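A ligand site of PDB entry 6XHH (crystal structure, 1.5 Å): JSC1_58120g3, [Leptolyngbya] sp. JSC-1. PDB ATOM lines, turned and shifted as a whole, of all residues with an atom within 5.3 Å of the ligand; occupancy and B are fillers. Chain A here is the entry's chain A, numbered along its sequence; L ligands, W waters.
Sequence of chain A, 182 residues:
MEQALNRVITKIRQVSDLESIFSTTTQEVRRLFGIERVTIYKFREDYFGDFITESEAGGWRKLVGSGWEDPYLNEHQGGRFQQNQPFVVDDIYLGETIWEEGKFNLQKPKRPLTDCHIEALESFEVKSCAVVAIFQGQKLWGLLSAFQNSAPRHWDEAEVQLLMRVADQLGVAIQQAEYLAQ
The side-chain sulfur (SG) of Cys 116 is bonded to a carbon (C5) of the ligand, 1.9 Å away. The backbone NH (N) of Thr 114 is in hydrogen-bond range of an oxygen (O3) of the ligand, 2.9 Å away. The side-chain hydroxyl (OG1) of Thr 114 is in hydrogen-bond range of an oxygen (O2) of the ligand (2.6 Å). The side-chain carboxylate of Asp 70 is in hydrogen-bond range of a nitrogen (N3) of the ligand, at 2.8 Å. The backbone NH (N) of Arg 80 sits at hydrogen-bond distance from an oxygen (O5) of the ligand, 2.9 Å away. NE of Arg 80 lies within salt-bridge range of O4 of the ligand (2.8 Å). OG of Ser 145 sits at hydrogen-bond distance from O6 of the ligand, at 2.8 Å. A ring nitrogen (ND1) of His 117 lies within hydrogen-bond range of an oxygen (O3) of the ligand (2.9 Å). An oxygen (O1) of the ligand is in hydrogen-bond range of the indole nitrogen of Trp 68 (2.9 Å).
The side-chain carboxylate of Asp 70 sits at hydrogen-bond distance from the backbone NH of Tyr 72. The side-chain carboxylate (OD1) of Asp 70 is in hydrogen-bond range of the backbone NH (N) of Leu 73, at 2.9 Å. O of Ser 145 lies within hydrogen-bond range of N of Thr 39. O of Trp 68 lies within hydrogen-bond range of OH of Tyr 41, 2.6 Å away. The backbone NH (N) of Val 131 is in hydrogen-bond range of the backbone carbonyl oxygen (O) of Phe 87 (2.8 Å). The backbone carbonyl oxygen of Tyr 41 sits at hydrogen-bond distance from the backbone NH of Leu 143. The backbone NH (N) of Gly 78 lies within hydrogen-bond range of the backbone carbonyl oxygen (O) of Leu 73 (2.8 Å).
CZ of Tyr 41 touches C29 of the ligand, at 3.5 Å. Phe 51 touches the ligand (CE1 to C33, 3.2 Å). CD of Pro 71 touches C1 of the ligand, at 3.3 Å. CG of Tyr 72 touches C12 of the ligand (3.4 Å). Leu 73 touches the ligand (CD2 to C21, 3.8 Å). CA of Gly 79 touches O5 of the ligand (3.6 Å). Phe 81 touches the ligand. Phe 87 touches the ligand (CD1 to C20, 3.8 Å). Leu 113 touches the ligand. Ala 120 touches the ligand (CB to O1, 3.4 Å). CG2 of Val 131 touches O6 of the ligand, at 3.2 Å. Leu 143 touches the ligand (CD1 to C31, 3.7 Å). Phe 147 touches the ligand. Hydrophobic or aromatic side chains within 4 Å of the ligand: Tyr 41, Phe 51, Trp 68, Pro 71, Tyr 72, Leu 73, Phe 81, Phe 87, Leu 113, His 117, Ala 120, Val 131, Leu 143 and Phe 147. The nearest printed residue that does not touch the ligand is Glu 69 (4.2 Å).
Water W3 lies within hydrogen-bond range of an oxygen (O4) of the ligand (2.6 Å) and the guanidinium group of Arg 80 (3.5 Å). Water W6 bridges the side-chain hydroxyl of Tyr 72 (2.6 Å) and an oxygen (O5) of the ligand (2.6 Å). Water W5 lies within hydrogen-bond range of an oxygen (O2) of the ligand (2.7 Å) and the side-chain hydroxyl of Thr 114 (3.4 Å). Water W2 bridges N4 of the ligand (2.8 Å) and NE2 of His 117 (2.9 Å). Water W7 lies within hydrogen-bond range of NH1 of Arg 111 (2.6 Å), O2 of the ligand (2.9 Å) and O of Pro 112 (2.9 Å).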
ATOM      1  N   THR A  39      24.253   2.984 -35.538  1.00  0.00           N
ATOM      2  CA  THR A  39      23.382   3.182 -36.688  1.00  0.00           C
ATOM      3  C   THR A  39      22.680   4.535 -36.611  1.00  0.00           C
ATOM      4  O   THR A  39      22.376   5.052 -35.524  1.00  0.00           O
ATOM      5  CB  THR A  39      22.291   2.100 -36.818  1.00  0.00           C
ATOM      6  OG1 THR A  39      21.433   2.119 -35.659  1.00  0.00           O
ATOM      7  CG2 THR A  39      22.897   0.741 -36.951  1.00  0.00           C
ATOM      8  N   TYR A  41      19.054   5.806 -38.079  1.00  0.00           N
ATOM      9  CA  TYR A  41      17.798   5.246 -38.534  1.00  0.00           C
ATOM     10  C   TYR A  41      16.815   6.395 -38.727  1.00  0.00           C
ATOM     11  O   TYR A  41      16.686   7.252 -37.848  1.00  0.00           O
ATOM     12  CB  TYR A  41      17.291   4.241 -37.501  1.00  0.00           C
ATOM     13  CG  TYR A  41      15.878   3.729 -37.566  1.00  0.00           C
ATOM     14  CD1 TYR A  41      14.835   4.451 -36.992  1.00  0.00           C
ATOM     15  CD2 TYR A  41      15.602   2.471 -38.060  1.00  0.00           C
ATOM     16  CE1 TYR A  41      13.543   3.958 -36.965  1.00  0.00           C
ATOM     17  CE2 TYR A  41      14.305   1.951 -38.048  1.00  0.00           C
ATOM     18  CZ  TYR A  41      13.283   2.710 -37.482  1.00  0.00           C
ATOM     19  OH  TYR A  41      12.007   2.201 -37.464  1.00  0.00           O
ATOM     20  N   PHE A  51      17.077   1.786 -41.692  1.00  0.00           N
ATOM     21  CA  PHE A  51      18.485   2.037 -41.394  1.00  0.00           C
ATOM     22  C   PHE A  51      19.147   2.772 -42.567  1.00  0.00           C
ATOM     23  O   PHE A  51      19.200   2.242 -43.692  1.00  0.00           O
ATOM     24  CB  PHE A  51      19.201   0.718 -41.124  1.00  0.00           C
ATOM     25  CG  PHE A  51      18.761   0.025 -39.883  1.00  0.00           C
ATOM     26  CD1 PHE A  51      19.321   0.353 -38.655  1.00  0.00           C
ATOM     27  CD2 PHE A  51      17.780  -0.952 -39.930  1.00  0.00           C
ATOM     28  CE1 PHE A  51      18.925  -0.297 -37.493  1.00  0.00           C
ATOM     29  CE2 PHE A  51      17.353  -1.603 -38.777  1.00  0.00           C
ATOM     30  CZ  PHE A  51      17.934  -1.279 -37.562  1.00  0.00           C
ATOM     31  N   TRP A  68      12.824  -1.407 -39.840  1.00  0.00           N
ATOM     32  CA  TRP A  68      12.230  -1.911 -38.597  1.00  0.00           C
ATOM     33  C   TRP A  68      10.902  -1.204 -38.447  1.00  0.00           C
ATOM     34  O   TRP A  68      10.848   0.018 -38.275  1.00  0.00           O
ATOM     35  CB  TRP A  68      13.162  -1.653 -37.413  1.00  0.00           C
ATOM     36  CG  TRP A  68      12.709  -2.167 -36.077  1.00  0.00           C
ATOM     37  CD1 TRP A  68      11.481  -2.658 -35.746  1.00  0.00           C
ATOM     38  CD2 TRP A  68      13.515  -2.243 -34.905  1.00  0.00           C
ATOM     39  NE1 TRP A  68      11.469  -3.035 -34.407  1.00  0.00           N
ATOM     40  CE2 TRP A  68      12.712  -2.789 -33.878  1.00  0.00           C
ATOM     41  CE3 TRP A  68      14.841  -1.915 -34.619  1.00  0.00           C
ATOM     42  CZ2 TRP A  68      13.214  -3.002 -32.588  1.00  0.00           C
ATOM     43  CZ3 TRP A  68      15.322  -2.112 -33.351  1.00  0.00           C
ATOM     44  CH2 TRP A  68      14.517  -2.647 -32.358  1.00  0.00           C
ATOM     45  N   GLU A  69       9.813  -1.978 -38.544  1.00  0.00           N
ATOM     46  CA  GLU A  69       8.450  -1.440 -38.414  1.00  0.00           C
ATOM     47  C   GLU A  69       7.965  -1.770 -37.007  1.00  0.00           C
ATOM     48  O   GLU A  69       7.283  -2.769 -36.765  1.00  0.00           O
ATOM     49  CB  GLU A  69       7.532  -2.008 -39.492  1.00  0.00           C
ATOM     50  CG  GLU A  69       8.058  -1.752 -40.916  1.00  0.00           C
ATOM     51  CD  GLU A  69       7.157  -2.305 -42.000  1.00  0.00           C
ATOM     52  OE1 GLU A  69       6.351  -3.223 -41.705  1.00  0.00           O
ATOM     53  OE2 GLU A  69       7.271  -1.832 -43.137  1.00  0.00           O
ATOM     54  N   ASP A  70       8.311  -0.898 -36.064  1.00  0.00           N
ATOM     55  CA  ASP A  70       7.987  -1.167 -34.675  1.00  0.00           C
ATOM     56  C   ASP A  70       6.549  -0.755 -34.393  1.00  0.00           C
ATOM     57  O   ASP A  70       6.227   0.429 -34.475  1.00  0.00           O
ATOM     58  CB  ASP A  70       8.921  -0.424 -33.729  1.00  0.00           C
ATOM     59  CG  ASP A  70       8.716  -0.844 -32.283  1.00  0.00           C
ATOM     60  OD1 ASP A  70       7.637  -0.512 -31.736  1.00  0.00           O
ATOM     61  OD2 ASP A  70       9.621  -1.471 -31.710  1.00  0.00           O
ATOM     62  N   PRO A  71       5.663  -1.695 -34.034  1.00  0.00           N
ATOM     63  CA  PRO A  71       4.244  -1.346 -33.843  1.00  0.00           C
ATOM     64  C   PRO A  71       4.013  -0.404 -32.689  1.00  0.00           C
ATOM     65  O   PRO A  71       3.065   0.392 -32.740  1.00  0.00           O
ATOM     66  CB  PRO A  71       3.581  -2.711 -33.580  1.00  0.00           C
ATOM     67  CG  PRO A  71       4.548  -3.728 -34.038  1.00  0.00           C
ATOM     68  CD  PRO A  71       5.906  -3.130 -33.844  1.00  0.00           C
ATOM     69  N   TYR A  72       4.831  -0.499 -31.646  1.00  0.00           N
ATOM     70  CA  TYR A  72       4.691   0.408 -30.508  1.00  0.00           C
ATOM     71  C   TYR A  72       5.050   1.838 -30.902  1.00  0.00           C
ATOM     72  O   TYR A  72       4.334   2.781 -30.561  1.00  0.00           O
ATOM     73  CB  TYR A  72       5.575  -0.076 -29.357  1.00  0.00           C
ATOM     74  CG  TYR A  72       5.458   0.768 -28.114  1.00  0.00           C
ATOM     75  CD1 TYR A  72       6.308   1.848 -27.893  1.00  0.00           C
ATOM     76  CD2 TYR A  72       4.504   0.479 -27.156  1.00  0.00           C
ATOM     77  CE1 TYR A  72       6.190   2.618 -26.749  1.00  0.00           C
ATOM     78  CE2 TYR A  72       4.384   1.257 -26.008  1.00  0.00           C
ATOM     79  CZ  TYR A  72       5.235   2.324 -25.807  1.00  0.00           C
ATOM     80  OH  TYR A  72       5.144   3.115 -24.685  1.00  0.00           O
ATOM     81  N   LEU A  73       6.183   2.006 -31.582  1.00  0.00           N
ATOM     82  CA  LEU A  73       6.565   3.343 -32.040  1.00  0.00           C
ATOM     83  C   LEU A  73       5.518   3.922 -33.004  1.00  0.00           C
ATOM     84  O   LEU A  73       5.296   5.139 -33.015  1.00  0.00           O
ATOM     85  CB  LEU A  73       7.948   3.297 -32.704  1.00  0.00           C
ATOM     86  CG  LEU A  73       9.146   2.981 -31.792  1.00  0.00           C
ATOM     87  CD1 LEU A  73      10.447   3.154 -32.508  1.00  0.00           C
ATOM     88  CD2 LEU A  73       9.139   3.835 -30.533  1.00  0.00           C
ATOM     89  N   GLY A  78       6.140   7.656 -32.160  1.00  0.00           N
ATOM     90  CA  GLY A  78       7.515   7.900 -31.760  1.00  0.00           C
ATOM     91  C   GLY A  78       7.818   7.614 -30.305  1.00  0.00           C
ATOM     92  O   GLY A  78       8.998   7.614 -29.927  1.00  0.00           O
ATOM     93  N   GLY A  79       6.803   7.374 -29.485  1.00  0.00           N
ATOM     94  CA  GLY A  79       7.031   6.997 -28.108  1.00  0.00           C
ATOM     95  C   GLY A  79       7.734   8.078 -27.318  1.00  0.00           C
ATOM     96  O   GLY A  79       7.509   9.271 -27.510  1.00  0.00           O
ATOM     97  N   ARG A  80       8.640   7.634 -26.432  1.00  0.00           N
ATOM     98  CA  ARG A  80       9.340   8.554 -25.546  1.00  0.00           C
ATOM     99  C   ARG A  80      10.245   9.512 -26.297  1.00  0.00           C
ATOM    100  O   ARG A  80      10.646  10.538 -25.727  1.00  0.00           O
ATOM    101  CB  ARG A  80      10.173   7.770 -24.535  1.00  0.00           C
ATOM    102  CG  ARG A  80      11.335   7.006 -25.187  1.00  0.00           C
ATOM    103  CD  ARG A  80      12.256   6.353 -24.148  1.00  0.00           C
ATOM    104  NE  ARG A  80      11.573   5.330 -23.361  1.00  0.00           N
ATOM    105  CZ  ARG A  80      12.015   4.897 -22.171  1.00  0.00           C
ATOM    106  NH1 ARG A  80      13.121   5.390 -21.642  1.00  0.00           N
ATOM    107  NH2 ARG A  80      11.328   3.980 -21.509  1.00  0.00           N
ATOM    108  N   PHE A  81      10.572   9.216 -27.556  1.00  0.00           N
ATOM    109  CA  PHE A  81      11.523  10.058 -28.262  1.00  0.00           C
ATOM    110  C   PHE A  81      10.924  11.421 -28.613  1.00  0.00           C
ATOM    111  O   PHE A  81      11.683  12.381 -28.832  1.00  0.00           O
ATOM    112  CB  PHE A  81      12.042   9.325 -29.501  1.00  0.00           C
ATOM    113  CG  PHE A  81      12.786   8.071 -29.157  1.00  0.00           C
ATOM    114  CD1 PHE A  81      14.006   8.148 -28.485  1.00  0.00           C
ATOM    115  CD2 PHE A  81      12.261   6.811 -29.437  1.00  0.00           C
ATOM    116  CE1 PHE A  81      14.687   7.006 -28.124  1.00  0.00           C
ATOM    117  CE2 PHE A  81      12.943   5.660 -29.079  1.00  0.00           C
ATOM    118  CZ  PHE A  81      14.162   5.764 -28.421  1.00  0.00           C
ATOM    119  N   PHE A  87      16.514   5.656 -24.499  1.00  0.00           N
ATOM    120  CA  PHE A  87      16.200   4.275 -24.168  1.00  0.00           C
ATOM    121  C   PHE A  87      17.515   3.531 -23.957  1.00  0.00           C
ATOM    122  O   PHE A  87      18.305   3.407 -24.897  1.00  0.00           O
ATOM    123  CB  PHE A  87      15.371   3.636 -25.280  1.00  0.00           C
ATOM    124  CG  PHE A  87      14.802   2.300 -24.939  1.00  0.00           C
ATOM    125  CD1 PHE A  87      13.887   2.164 -23.913  1.00  0.00           C
ATOM    126  CD2 PHE A  87      15.171   1.176 -25.650  1.00  0.00           C
ATOM    127  CE1 PHE A  87      13.350   0.945 -23.588  1.00  0.00           C
ATOM    128  CE2 PHE A  87      14.631  -0.056 -25.321  1.00  0.00           C
ATOM    129  CZ  PHE A  87      13.725  -0.175 -24.308  1.00  0.00           C
ATOM    130  N   ARG A 111      13.672  -2.309 -15.957  1.00  0.00           N
ATOM    131  CA  ARG A 111      12.328  -2.647 -16.415  1.00  0.00           C
ATOM    132  C   ARG A 111      12.402  -3.599 -17.606  1.00  0.00           C
ATOM    133  O   ARG A 111      12.836  -3.183 -18.688  1.00  0.00           O
ATOM    134  CB  ARG A 111      11.567  -1.380 -16.804  1.00  0.00           C
ATOM    135  CG  ARG A 111      10.112  -1.629 -17.158  1.00  0.00           C
ATOM    136  CD  ARG A 111       9.431  -0.312 -17.535  1.00  0.00           C
ATOM    137  NE  ARG A 111       8.013  -0.329 -17.206  1.00  0.00           N
ATOM    138  CZ  ARG A 111       7.052  -0.647 -18.062  1.00  0.00           C
ATOM    139  NH1 ARG A 111       7.350  -0.980 -19.319  1.00  0.00           N
ATOM    140  NH2 ARG A 111       5.782  -0.628 -17.681  1.00  0.00           N
ATOM    141  N   PRO A 112      11.973  -4.847 -17.465  1.00  0.00           N
ATOM    142  CA  PRO A 112      12.094  -5.812 -18.564  1.00  0.00           C
ATOM    143  C   PRO A 112      11.324  -5.389 -19.805  1.00  0.00           C
ATOM    144  O   PRO A 112      10.270  -4.765 -19.734  1.00  0.00           O
ATOM    145  CB  PRO A 112      11.515  -7.108 -17.967  1.00  0.00           C
ATOM    146  CG  PRO A 112      11.758  -6.971 -16.498  1.00  0.00           C
ATOM    147  CD  PRO A 112      11.541  -5.500 -16.214  1.00  0.00           C
ATOM    148  N   LEU A 113      11.882  -5.738 -20.966  1.00  0.00           N
ATOM    149  CA  LEU A 113      11.281  -5.433 -22.258  1.00  0.00           C
ATOM    150  C   LEU A 113      10.224  -6.475 -22.617  1.00  0.00           C
ATOM    151  O   LEU A 113      10.283  -7.623 -22.186  1.00  0.00           O
ATOM    152  CB  LEU A 113      12.343  -5.400 -23.356  1.00  0.00           C
ATOM    153  CG  LEU A 113      13.222  -4.154 -23.522  1.00  0.00           C
ATOM    154  CD1 LEU A 113      13.945  -3.740 -22.258  1.00  0.00           C
ATOM    155  CD2 LEU A 113      14.223  -4.413 -24.634  1.00  0.00           C
ATOM    156  N   THR A 114       9.256  -6.054 -23.428  1.00  0.00           N
ATOM    157  CA  THR A 114       8.254  -6.966 -23.964  1.00  0.00           C
ATOM    158  C   THR A 114       8.910  -7.968 -24.915  1.00  0.00           C
ATOM    159  O   THR A 114       9.861  -7.630 -25.608  1.00  0.00           O
ATOM    160  CB  THR A 114       7.182  -6.148 -24.700  1.00  0.00           C
ATOM    161  OG1 THR A 114       6.466  -5.334 -23.755  1.00  0.00           O
ATOM    162  CG2 THR A 114       6.216  -7.030 -25.469  1.00  0.00           C
ATOM    163  N   CYS A 116       8.224  -9.414 -27.778  1.00  0.00           N
ATOM    164  CA  CYS A 116       8.331  -9.159 -29.221  1.00  0.00           C
ATOM    165  C   CYS A 116       9.322  -8.048 -29.537  1.00  0.00           C
ATOM    166  O   CYS A 116       9.917  -8.044 -30.622  1.00  0.00           O
ATOM    167  CB  CYS A 116       6.955  -8.848 -29.846  1.00  0.00           C
ATOM    168  SG  CYS A 116       6.002  -7.442 -29.273  1.00  0.00           S
ATOM    169  N   HIS A 117       9.507  -7.102 -28.596  1.00  0.00           N
ATOM    170  CA  HIS A 117      10.589  -6.133 -28.703  1.00  0.00           C
ATOM    171  C   HIS A 117      11.933  -6.840 -28.622  1.00  0.00           C
ATOM    172  O   HIS A 117      12.819  -6.631 -29.468  1.00  0.00           O
ATOM    173  CB  HIS A 117      10.419  -5.094 -27.593  1.00  0.00           C
ATOM    174  CG  HIS A 117      11.374  -3.941 -27.668  1.00  0.00           C
ATOM    175  ND1 HIS A 117      11.324  -2.901 -26.759  1.00  0.00           N
ATOM    176  CD2 HIS A 117      12.389  -3.648 -28.518  1.00  0.00           C
ATOM    177  CE1 HIS A 117      12.269  -2.018 -27.051  1.00  0.00           C
ATOM    178  NE2 HIS A 117      12.925  -2.450 -28.115  1.00  0.00           N
ATOM    179  N   ALA A 120      12.557  -8.659 -31.878  1.00  0.00           N
ATOM    180  CA  ALA A 120      12.964  -7.700 -32.910  1.00  0.00           C
ATOM    181  C   ALA A 120      14.440  -7.340 -32.777  1.00  0.00           C
ATOM    182  O   ALA A 120      15.180  -7.326 -33.770  1.00  0.00           O
ATOM    183  CB  ALA A 120      12.102  -6.448 -32.819  1.00  0.00           C
ATOM    184  N   LEU A 121      14.895  -7.078 -31.559  1.00  0.00           N
ATOM    185  CA  LEU A 121      16.308  -6.795 -31.322  1.00  0.00           C
ATOM    186  C   LEU A 121      17.192  -7.981 -31.692  1.00  0.00           C
ATOM    187  O   LEU A 121      18.223  -7.809 -32.362  1.00  0.00           O
ATOM    188  CB  LEU A 121      16.507  -6.390 -29.845  1.00  0.00           C
ATOM    189  CG  LEU A 121      15.974  -4.998 -29.491  1.00  0.00           C
ATOM    190  CD1 LEU A 121      15.722  -4.814 -27.995  1.00  0.00           C
ATOM    191  CD2 LEU A 121      16.937  -3.951 -30.009  1.00  0.00           C
ATOM    192  N   CYS A 129      21.558  -2.000 -26.047  1.00  0.00           N
ATOM    193  CA  CYS A 129      21.312  -0.843 -26.902  1.00  0.00           C
ATOM    194  C   CYS A 129      21.149   0.425 -26.087  1.00  0.00           C
ATOM    195  O   CYS A 129      20.487   0.427 -25.046  1.00  0.00           O
ATOM    196  CB  CYS A 129      20.050  -1.018 -27.775  1.00  0.00           C
ATOM    197  SG  CYS A 129      18.506  -1.388 -26.861  1.00  0.00           S
ATOM    198  N   VAL A 131      19.774   4.203 -27.177  1.00  0.00           N
ATOM    199  CA  VAL A 131      19.046   4.750 -28.322  1.00  0.00           C
ATOM    200  C   VAL A 131      18.560   6.153 -27.983  1.00  0.00           C
ATOM    201  O   VAL A 131      17.953   6.370 -26.926  1.00  0.00           O
ATOM    202  CB  VAL A 131      17.857   3.855 -28.735  1.00  0.00           C
ATOM    203  CG1 VAL A 131      17.253   4.316 -30.077  1.00  0.00           C
ATOM    204  CG2 VAL A 131      18.276   2.378 -28.817  1.00  0.00           C
ATOM    205  N   LEU A 143      16.524   8.092 -35.191  1.00  0.00           N
ATOM    206  CA  LEU A 143      17.186   7.583 -33.997  1.00  0.00           C
ATOM    207  C   LEU A 143      18.654   7.322 -34.270  1.00  0.00           C
ATOM    208  O   LEU A 143      19.009   6.818 -35.342  1.00  0.00           O
ATOM    209  CB  LEU A 143      16.518   6.287 -33.500  1.00  0.00           C
ATOM    210  CG  LEU A 143      15.009   6.336 -33.245  1.00  0.00           C
ATOM    211  CD1 LEU A 143      14.443   4.939 -33.006  1.00  0.00           C
ATOM    212  CD2 LEU A 143      14.718   7.237 -32.059  1.00  0.00           C
ATOM    213  N   SER A 145      21.505   4.969 -32.609  1.00  0.00           N
ATOM    214  CA  SER A 145      21.574   3.779 -31.762  1.00  0.00           C
ATOM    215  C   SER A 145      23.021   3.319 -31.645  1.00  0.00           C
ATOM    216  O   SER A 145      23.721   3.193 -32.649  1.00  0.00           O
ATOM    217  CB  SER A 145      20.706   2.624 -32.311  1.00  0.00           C
ATOM    218  OG  SER A 145      19.352   3.055 -32.428  1.00  0.00           O
ATOM    219  N   PHE A 147      24.960  -0.037 -30.303  1.00  0.00           N
ATOM    220  CA  PHE A 147      24.619  -1.439 -30.078  1.00  0.00           C
ATOM    221  C   PHE A 147      25.857  -2.235 -29.684  1.00  0.00           C
ATOM    222  O   PHE A 147      26.955  -2.027 -30.214  1.00  0.00           O
ATOM    223  CB  PHE A 147      24.041  -2.084 -31.354  1.00  0.00           C
ATOM    224  CG  PHE A 147      22.700  -1.550 -31.805  1.00  0.00           C
ATOM    225  CD1 PHE A 147      21.642  -1.380 -30.926  1.00  0.00           C
ATOM    226  CD2 PHE A 147      22.495  -1.264 -33.154  1.00  0.00           C
ATOM    227  CE1 PHE A 147      20.397  -0.935 -31.388  1.00  0.00           C
ATOM    228  CE2 PHE A 147      21.262  -0.807 -33.615  1.00  0.00           C
ATOM    229  CZ  PHE A 147      20.222  -0.648 -32.728  1.00  0.00           C
HETATM  230  O1  LIG L   1       9.246  -4.730 -33.546  1.00  0.00           O
HETATM  231  C1  LIG L   1       8.447  -4.878 -32.625  1.00  0.00           C
HETATM  232  N1  LIG L   1       8.413  -4.099 -31.534  1.00  0.00           N
HETATM  233  C2  LIG L   1       7.430  -5.844 -32.562  1.00  0.00           C
HETATM  234  C3  LIG L   1       7.149  -6.906 -33.608  1.00  0.00           C
HETATM  235  C4  LIG L   1       6.747  -5.675 -31.360  1.00  0.00           C
HETATM  236  C5  LIG L   1       5.608  -6.467 -30.853  1.00  0.00           C
HETATM  237  C6  LIG L   1       4.344  -5.623 -30.676  1.00  0.00           C
HETATM  238  C7  LIG L   1       7.389  -4.531 -30.687  1.00  0.00           C
HETATM  239  C8  LIG L   1       7.003  -4.014 -29.476  1.00  0.00           C
HETATM  240  C9  LIG L   1       7.522  -2.894 -28.693  1.00  0.00           C
HETATM  241  C10 LIG L   1       6.996  -2.577 -27.420  1.00  0.00           C
HETATM  242  C11 LIG L   1       5.894  -3.315 -26.709  1.00  0.00           C
HETATM  243  C12 LIG L   1       7.683  -1.497 -26.951  1.00  0.00           C
HETATM  244  C13 LIG L   1       7.480  -0.804 -25.614  1.00  0.00           C
HETATM  245  C14 LIG L   1       8.642  -1.127 -24.665  1.00  0.00           C
HETATM  246  C15 LIG L   1       8.591  -2.583 -24.250  1.00  0.00           C
HETATM  247  O2  LIG L   1       7.655  -2.997 -23.515  1.00  0.00           O
HETATM  248  O3  LIG L   1       9.467  -3.398 -24.619  1.00  0.00           O
HETATM  249  N2  LIG L   1       8.504  -2.015 -28.986  1.00  0.00           N
HETATM  250  C16 LIG L   1       8.631  -1.148 -27.965  1.00  0.00           C
HETATM  251  C17 LIG L   1       9.505  -0.061 -27.816  1.00  0.00           C
HETATM  252  C18 LIG L   1      10.632   0.348 -28.549  1.00  0.00           C
HETATM  253  C19 LIG L   1      11.551   1.281 -28.049  1.00  0.00           C
HETATM  254  C20 LIG L   1      11.411   2.010 -26.730  1.00  0.00           C
HETATM  255  C21 LIG L   1      10.433   3.171 -27.057  1.00  0.00           C
HETATM  256  C22 LIG L   1       9.755   3.822 -25.860  1.00  0.00           C
HETATM  257  O4  LIG L   1      10.006   3.437 -24.703  1.00  0.00           O
HETATM  258  O5  LIG L   1       8.912   4.734 -26.021  1.00  0.00           O
HETATM  259  C23 LIG L   1      12.524   1.453 -29.031  1.00  0.00           C
HETATM  260  C24 LIG L   1      13.704   2.380 -28.908  1.00  0.00           C
HETATM  261  N3  LIG L   1      11.049  -0.057 -29.794  1.00  0.00           N
HETATM  262  C25 LIG L   1      12.205   0.596 -30.104  1.00  0.00           C
HETATM  263  C26 LIG L   1      12.825   0.364 -31.365  1.00  0.00           C
HETATM  264  C27 LIG L   1      14.059   0.745 -31.843  1.00  0.00           C
HETATM  265  C28 LIG L   1      14.327   1.206 -33.162  1.00  0.00           C
HETATM  266  C29 LIG L   1      13.298   1.404 -34.254  1.00  0.00           C
HETATM  267  N4  LIG L   1      15.257   0.686 -31.155  1.00  0.00           N
HETATM  268  C30 LIG L   1      16.240   1.124 -31.976  1.00  0.00           C
HETATM  269  O6  LIG L   1      17.424   1.180 -31.635  1.00  0.00           O
HETATM  270  C31 LIG L   1      15.659   1.456 -33.242  1.00  0.00           C
HETATM  271  C32 LIG L   1      16.390   1.999 -34.450  1.00  0.00           C
HETATM  272  C33 LIG L   1      17.153   0.876 -35.121  1.00  0.00           C
HETATM  273  O   HOH W   1       9.332  -9.451 -32.959  1.00  0.00           O
HETATM  274  O   HOH W   2      15.238  -0.794 -28.789  1.00  0.00           O
HETATM  275  O   HOH W   3       9.389   1.523 -23.045  1.00  0.00           O
HETATM  276  O   HOH W   4       9.698  -6.350 -36.135  1.00  0.00           O
HETATM  277  O   HOH W   5       5.040  -2.314 -23.401  1.00  0.00           O
HETATM  278  O   HOH W   6       6.775   5.155 -24.514  1.00  0.00           O
HETATM  279  O   HOH W   7       8.691  -2.635 -20.856  1.00  0.00           O
